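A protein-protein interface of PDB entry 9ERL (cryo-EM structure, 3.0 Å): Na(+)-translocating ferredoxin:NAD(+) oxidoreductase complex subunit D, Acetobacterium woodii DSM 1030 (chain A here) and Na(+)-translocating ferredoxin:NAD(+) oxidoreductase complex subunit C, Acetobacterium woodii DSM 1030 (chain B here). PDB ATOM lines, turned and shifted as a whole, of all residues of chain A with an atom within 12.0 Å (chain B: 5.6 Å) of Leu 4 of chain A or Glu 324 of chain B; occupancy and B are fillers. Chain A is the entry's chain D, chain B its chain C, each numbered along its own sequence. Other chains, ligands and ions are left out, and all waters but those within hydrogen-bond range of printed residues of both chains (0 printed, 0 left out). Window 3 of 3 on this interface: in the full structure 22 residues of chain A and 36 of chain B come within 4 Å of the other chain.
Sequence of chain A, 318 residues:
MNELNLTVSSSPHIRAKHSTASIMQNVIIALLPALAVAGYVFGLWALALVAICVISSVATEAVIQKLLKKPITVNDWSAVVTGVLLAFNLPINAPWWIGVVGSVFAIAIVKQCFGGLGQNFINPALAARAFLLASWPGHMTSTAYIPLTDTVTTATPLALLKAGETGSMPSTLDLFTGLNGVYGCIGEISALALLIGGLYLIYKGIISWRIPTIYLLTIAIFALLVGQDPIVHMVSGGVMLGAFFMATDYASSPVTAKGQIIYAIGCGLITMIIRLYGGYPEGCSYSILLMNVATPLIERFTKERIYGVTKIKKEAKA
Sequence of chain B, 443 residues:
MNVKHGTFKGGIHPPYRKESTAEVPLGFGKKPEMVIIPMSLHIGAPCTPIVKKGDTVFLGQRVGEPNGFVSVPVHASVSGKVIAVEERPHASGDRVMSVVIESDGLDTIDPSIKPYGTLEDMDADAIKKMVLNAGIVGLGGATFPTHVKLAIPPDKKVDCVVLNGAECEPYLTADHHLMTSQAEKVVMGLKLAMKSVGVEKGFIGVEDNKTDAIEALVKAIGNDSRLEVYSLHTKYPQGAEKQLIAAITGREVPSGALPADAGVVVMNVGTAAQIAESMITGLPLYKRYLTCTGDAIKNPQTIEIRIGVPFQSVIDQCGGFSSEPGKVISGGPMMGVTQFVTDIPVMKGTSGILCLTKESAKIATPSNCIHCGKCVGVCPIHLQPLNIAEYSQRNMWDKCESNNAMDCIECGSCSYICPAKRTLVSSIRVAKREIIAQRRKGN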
ATOM      1  N   MET A   1     -14.303 -16.530  30.732  1.00  0.00           N
ATOM      2  CA  MET A   1     -13.287 -17.402  30.155  1.00  0.00           C
ATOM      3  C   MET A   1     -13.618 -18.864  30.443  1.00  0.00           C
ATOM      4  O   MET A   1     -12.828 -19.585  31.053  1.00  0.00           O
ATOM      5  CB  MET A   1     -11.903 -17.047  30.704  1.00  0.00           C
ATOM      6  CG  MET A   1     -10.744 -17.461  29.806  1.00  0.00           C
ATOM      7  SD  MET A   1      -9.294 -16.401  29.983  1.00  0.00           S
ATOM      8  CE  MET A   1      -9.466 -15.846  31.678  1.00  0.00           C
ATOM      9  N   ASN A   2     -14.798 -19.293  30.006  1.00  0.00           N
ATOM     10  CA  ASN A   2     -15.240 -20.660  30.236  1.00  0.00           C
ATOM     11  C   ASN A   2     -14.893 -21.544  29.045  1.00  0.00           C
ATOM     12  O   ASN A   2     -15.149 -21.190  27.891  1.00  0.00           O
ATOM     13  CB  ASN A   2     -16.747 -20.699  30.495  1.00  0.00           C
ATOM     14  CG  ASN A   2     -17.534 -19.893  29.482  1.00  0.00           C
ATOM     15  OD1 ASN A   2     -16.973 -19.089  28.738  1.00  0.00           O
ATOM     16  ND2 ASN A   2     -18.845 -20.107  29.446  1.00  0.00           N
ATOM     17  N   GLU A   3     -14.306 -22.701  29.335  1.00  0.00           N
ATOM     18  CA  GLU A   3     -13.952 -23.671  28.314  1.00  0.00           C
ATOM     19  C   GLU A   3     -15.030 -24.748  28.231  1.00  0.00           C
ATOM     20  O   GLU A   3     -16.040 -24.713  28.939  1.00  0.00           O
ATOM     21  CB  GLU A   3     -12.579 -24.280  28.605  1.00  0.00           C
ATOM     22  CG  GLU A   3     -11.433 -23.279  28.586  1.00  0.00           C
ATOM     23  CD  GLU A   3     -10.807 -23.122  27.213  1.00  0.00           C
ATOM     24  OE1 GLU A   3     -11.555 -23.007  26.219  1.00  0.00           O
ATOM     25  OE2 GLU A   3      -9.562 -23.114  27.127  1.00  0.00           O
ATOM     26  N   LEU A   4     -14.808 -25.722  27.353  1.00  0.00           N
ATOM     27  CA  LEU A   4     -15.757 -26.807  27.149  1.00  0.00           C
ATOM     28  C   LEU A   4     -15.175 -28.165  27.509  1.00  0.00           C
ATOM     29  O   LEU A   4     -15.822 -28.935  28.230  1.00  0.00           O
ATOM     30  CB  LEU A   4     -16.245 -26.807  25.691  1.00  0.00           C
ATOM     31  CG  LEU A   4     -17.407 -25.862  25.370  1.00  0.00           C
ATOM     32  CD1 LEU A   4     -17.911 -26.085  23.954  1.00  0.00           C
ATOM     33  CD2 LEU A   4     -18.535 -26.033  26.374  1.00  0.00           C
ATOM     34  N   ASN A   5     -13.964 -28.469  27.033  1.00  0.00           N
ATOM     35  CA  ASN A   5     -13.277 -29.739  27.287  1.00  0.00           C
ATOM     36  C   ASN A   5     -14.146 -30.931  26.880  1.00  0.00           C
ATOM     37  O   ASN A   5     -14.560 -31.750  27.703  1.00  0.00           O
ATOM     38  CB  ASN A   5     -12.833 -29.850  28.750  1.00  0.00           C
ATOM     39  CG  ASN A   5     -11.574 -30.681  28.913  1.00  0.00           C
ATOM     40  OD1 ASN A   5     -11.568 -31.689  29.618  1.00  0.00           O
ATOM     41  ND2 ASN A   5     -10.497 -30.260  28.260  1.00  0.00           N
ATOM     42  N   LEU A   6     -14.421 -31.008  25.583  1.00  0.00           N
ATOM     43  CA  LEU A   6     -15.250 -32.071  25.045  1.00  0.00           C
ATOM     44  C   LEU A   6     -14.443 -33.361  24.917  1.00  0.00           C
ATOM     45  O   LEU A   6     -13.254 -33.422  25.239  1.00  0.00           O
ATOM     46  CB  LEU A   6     -15.829 -31.655  23.695  1.00  0.00           C
ATOM     47  CG  LEU A   6     -16.489 -30.274  23.667  1.00  0.00           C
ATOM     48  CD1 LEU A   6     -16.814 -29.859  22.245  1.00  0.00           C
ATOM     49  CD2 LEU A   6     -17.740 -30.261  24.524  1.00  0.00           C
ATOM     50  N   THR A   7     -15.108 -34.408  24.440  1.00  0.00           N
ATOM     51  CA  THR A   7     -14.499 -35.714  24.244  1.00  0.00           C
ATOM     52  C   THR A   7     -14.433 -36.026  22.756  1.00  0.00           C
ATOM     53  O   THR A   7     -15.386 -35.768  22.016  1.00  0.00           O
ATOM     54  CB  THR A   7     -15.289 -36.804  24.974  1.00  0.00           C
ATOM     55  OG1 THR A   7     -15.575 -36.374  26.310  1.00  0.00           O
ATOM     56  CG2 THR A   7     -14.498 -38.100  25.027  1.00  0.00           C
ATOM     57  N   VAL A   8     -13.300 -36.571  22.319  1.00  0.00           N
ATOM     58  CA  VAL A   8     -13.088 -36.942  20.925  1.00  0.00           C
ATOM     59  C   VAL A   8     -12.848 -38.443  20.858  1.00  0.00           C
ATOM     60  O   VAL A   8     -12.043 -38.985  21.624  1.00  0.00           O
ATOM     61  CB  VAL A   8     -11.917 -36.165  20.296  1.00  0.00           C
ATOM     62  CG1 VAL A   8     -12.371 -34.779  19.884  1.00  0.00           C
ATOM     63  CG2 VAL A   8     -10.749 -36.070  21.259  1.00  0.00           C
ATOM     64  N   ALA B 296     -28.650 -31.737  24.908  1.00  0.00           N
ATOM     65  CA  ALA B 296     -28.290 -30.493  25.575  1.00  0.00           C
ATOM     66  C   ALA B 296     -28.777 -29.268  24.806  1.00  0.00           C
ATOM     67  O   ALA B 296     -28.176 -28.196  24.892  1.00  0.00           O
ATOM     68  CB  ALA B 296     -26.779 -30.420  25.787  1.00  0.00           C
ATOM     69  N   PHE B 321     -27.703 -23.974  25.394  1.00  0.00           N
ATOM     70  CA  PHE B 321     -27.388 -25.188  26.137  1.00  0.00           C
ATOM     71  C   PHE B 321     -28.179 -25.198  27.440  1.00  0.00           C
ATOM     72  O   PHE B 321     -28.045 -24.282  28.258  1.00  0.00           O
ATOM     73  CB  PHE B 321     -25.890 -25.281  26.429  1.00  0.00           C
ATOM     74  CG  PHE B 321     -25.055 -25.638  25.233  1.00  0.00           C
ATOM     75  CD1 PHE B 321     -25.384 -26.719  24.436  1.00  0.00           C
ATOM     76  CD2 PHE B 321     -23.929 -24.898  24.916  1.00  0.00           C
ATOM     77  CE1 PHE B 321     -24.613 -27.050  23.340  1.00  0.00           C
ATOM     78  CE2 PHE B 321     -23.153 -25.224  23.823  1.00  0.00           C
ATOM     79  CZ  PHE B 321     -23.496 -26.301  23.034  1.00  0.00           C
ATOM     80  N   SER B 322     -28.999 -26.233  27.631  1.00  0.00           N
ATOM     81  CA  SER B 322     -29.690 -26.390  28.906  1.00  0.00           C
ATOM     82  C   SER B 322     -28.739 -26.873  29.993  1.00  0.00           C
ATOM     83  O   SER B 322     -28.940 -26.567  31.174  1.00  0.00           O
ATOM     84  CB  SER B 322     -30.864 -27.356  28.758  1.00  0.00           C
ATOM     85  OG  SER B 322     -30.432 -28.609  28.261  1.00  0.00           O
ATOM     86  N   SER B 323     -27.708 -27.624  29.614  1.00  0.00           N
ATOM     87  CA  SER B 323     -26.682 -28.085  30.536  1.00  0.00           C
ATOM     88  C   SER B 323     -25.349 -28.103  29.801  1.00  0.00           C
ATOM     89  O   SER B 323     -25.276 -27.837  28.599  1.00  0.00           O
ATOM     90  CB  SER B 323     -27.014 -29.471  31.102  1.00  0.00           C
ATOM     91  OG  SER B 323     -27.083 -30.439  30.071  1.00  0.00           O
ATOM     92  N   GLU B 324     -24.290 -28.415  30.533  1.00  0.00           N
ATOM     93  CA  GLU B 324     -22.956 -28.443  29.943  1.00  0.00           C
ATOM     94  C   GLU B 324     -22.826 -29.639  29.010  1.00  0.00           C
ATOM     95  O   GLU B 324     -23.012 -30.780  29.453  1.00  0.00           O
ATOM     96  CB  GLU B 324     -21.893 -28.500  31.033  1.00  0.00           C
ATOM     97  CG  GLU B 324     -20.677 -27.633  30.753  1.00  0.00           C
ATOM     98  CD  GLU B 324     -19.483 -28.006  31.610  1.00  0.00           C
ATOM     99  OE1 GLU B 324     -19.676 -28.281  32.813  1.00  0.00           O
ATOM    100  OE2 GLU B 324     -18.352 -28.023  31.081  1.00  0.00           O
ATOM    101  N   PRO B 325     -22.518 -29.437  27.730  1.00  0.00           N
ATOM    102  CA  PRO B 325     -22.402 -30.574  26.814  1.00  0.00           C
ATOM    103  C   PRO B 325     -21.120 -31.354  27.047  1.00  0.00           C
ATOM    104  O   PRO B 325     -20.125 -30.830  27.552  1.00  0.00           O
ATOM    105  CB  PRO B 325     -22.406 -29.914  25.433  1.00  0.00           C
ATOM    106  CG  PRO B 325     -21.829 -28.567  25.672  1.00  0.00           C
ATOM    107  CD  PRO B 325     -22.251 -28.153  27.059  1.00  0.00           C
ATOM    108  N   GLY B 326     -21.157 -32.627  26.670  1.00  0.00           N
ATOM    109  CA  GLY B 326     -19.989 -33.476  26.780  1.00  0.00           C
ATOM    110  C   GLY B 326     -19.475 -33.953  25.439  1.00  0.00           C
ATOM    111  O   GLY B 326     -18.415 -34.579  25.364  1.00  0.00           O
ATOM    112  N   VAL B 328     -19.947 -32.792  21.000  1.00  0.00           N
ATOM    113  CA  VAL B 328     -20.558 -32.072  19.886  1.00  0.00           C
ATOM    114  C   VAL B 328     -20.181 -32.801  18.605  1.00  0.00           C
ATOM    115  O   VAL B 328     -18.993 -33.011  18.334  1.00  0.00           O
ATOM    116  CB  VAL B 328     -20.112 -30.602  19.837  1.00  0.00           C
ATOM    117  CG1 VAL B 328     -20.715 -29.905  18.631  1.00  0.00           C
ATOM    118  CG2 VAL B 328     -20.502 -29.886  21.117  1.00  0.00           C
ATOM    119  N   THR B 342     -16.272 -24.631  18.705  1.00  0.00           N
ATOM    120  CA  THR B 342     -17.559 -24.249  18.137  1.00  0.00           C
ATOM    121  C   THR B 342     -17.439 -23.102  17.138  1.00  0.00           C
ATOM    122  O   THR B 342     -18.443 -22.468  16.805  1.00  0.00           O
ATOM    123  CB  THR B 342     -18.542 -23.877  19.247  1.00  0.00           C
ATOM    124  OG1 THR B 342     -17.841 -23.220  20.309  1.00  0.00           O
ATOM    125  CG2 THR B 342     -19.228 -25.119  19.791  1.00  0.00           C
ATOM    126  N   LEU B 356     -24.588 -33.831  22.932  1.00  0.00           N
ATOM    127  CA  LEU B 356     -24.908 -34.791  23.977  1.00  0.00           C
ATOM    128  C   LEU B 356     -24.396 -34.296  25.322  1.00  0.00           C
ATOM    129  O   LEU B 356     -23.375 -33.609  25.410  1.00  0.00           O
ATOM    130  CB  LEU B 356     -24.305 -36.166  23.668  1.00  0.00           C
ATOM    131  CG  LEU B 356     -24.744 -36.856  22.377  1.00  0.00           C
ATOM    132  CD1 LEU B 356     -24.018 -38.177  22.216  1.00  0.00           C
ATOM    133  CD2 LEU B 356     -26.247 -37.064  22.365  1.00  0.00           C
ATOM    134  N   THR B 357     -25.121 -34.655  26.376  1.00  0.00           N
ATOM    135  CA  THR B 357     -24.745 -34.273  27.725  1.00  0.00           C
ATOM    136  C   THR B 357     -23.647 -35.202  28.242  1.00  0.00           C
ATOM    137  O   THR B 357     -23.235 -36.153  27.574  1.00  0.00           O
ATOM    138  CB  THR B 357     -25.965 -34.282  28.644  1.00  0.00           C
ATOM    139  OG1 THR B 357     -25.647 -33.613  29.870  1.00  0.00           O
ATOM    140  CG2 THR B 357     -26.395 -35.703  28.948  1.00  0.00           C
ATOM    141  N   LYS B 358     -23.156 -34.915  29.451  1.00  0.00           N
ATOM    142  CA  LYS B 358     -22.044 -35.680  30.007  1.00  0.00           C
ATOM    143  C   LYS B 358     -22.448 -37.107  30.354  1.00  0.00           C
ATOM    144  O   LYS B 358     -21.626 -38.024  30.250  1.00  0.00           O
ATOM    145  CB  LYS B 358     -21.491 -34.973  31.243  1.00  0.00           C
ATOM    146  CG  LYS B 358     -20.380 -33.985  30.942  1.00  0.00           C
ATOM    147  CD  LYS B 358     -19.988 -33.203  32.183  1.00  0.00           C
ATOM    148  CE  LYS B 358     -19.411 -31.846  31.821  1.00  0.00           C
ATOM    149  NZ  LYS B 358     -18.217 -31.971  30.942  1.00  0.00           N
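O of Gly 326 of chain B sits at hydrogen-bond distance from N of Thr 7 of chain A.
NZ of Lys 358 of chain B is in salt-bridge range of OE2 of Glu 324 of chain B.
N of Gly 326 of chain B lies within hydrogen-bond range of O of Leu 356 of chain B (2.7 Å).
Among the printed residues, merely in contact across the chains: Leu 4 of chain A with Glu 324 of chain B (3.9 Å), Leu 6 of chain A with Pro 325 of chain B (3.9 Å) and Leu 6 of chain A with Val 328 of chain B (3.9 Å).
Leu 4 of chain A touches one residue of chain B.
Printed residues of chain A within 4 Å of Glu 324 of chain B: Leu 4 (3.9 Å).
No residue of chain A comes within 4 Å of Phe 321 of chain B.
No residue of chain A comes within 4 Å of Ser 323 of chain B.
Of chain A, only Leu 6 (3.9 Å) comes within 4 Å of Pro 325 of chain B.
Of chain A, only Thr 7 (3.4 Å) comes within 4 Å of Gly 326 of chain B.
No residue of chain A comes within 4 Å of Lys 358 of chain B.
Printed residues of chain B within 4 Å of Thr 7 of chain A: Gly 326 (3.4 Å).
Of the printed residues of chain B, Leu 6 of chain A touches Pro 325 and Val 328.
Of the printed residues of chain A, Val 328 of chain B touches Leu 6 (3.9 Å).
Of the 12 printed residues of chain B, 4 touch a printed residue of chain A.
Printed residues of chain B that touch a printed residue of chain A: Glu 324, Pro 325, Gly 326 and Val 328.
Hydrophobic or aromatic side chains of chain B within 4 Å of the printed part of chain A: Val 328.
Hydrophobic or aromatic side chains of chain A that line the printed part of chain B: Leu 6.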
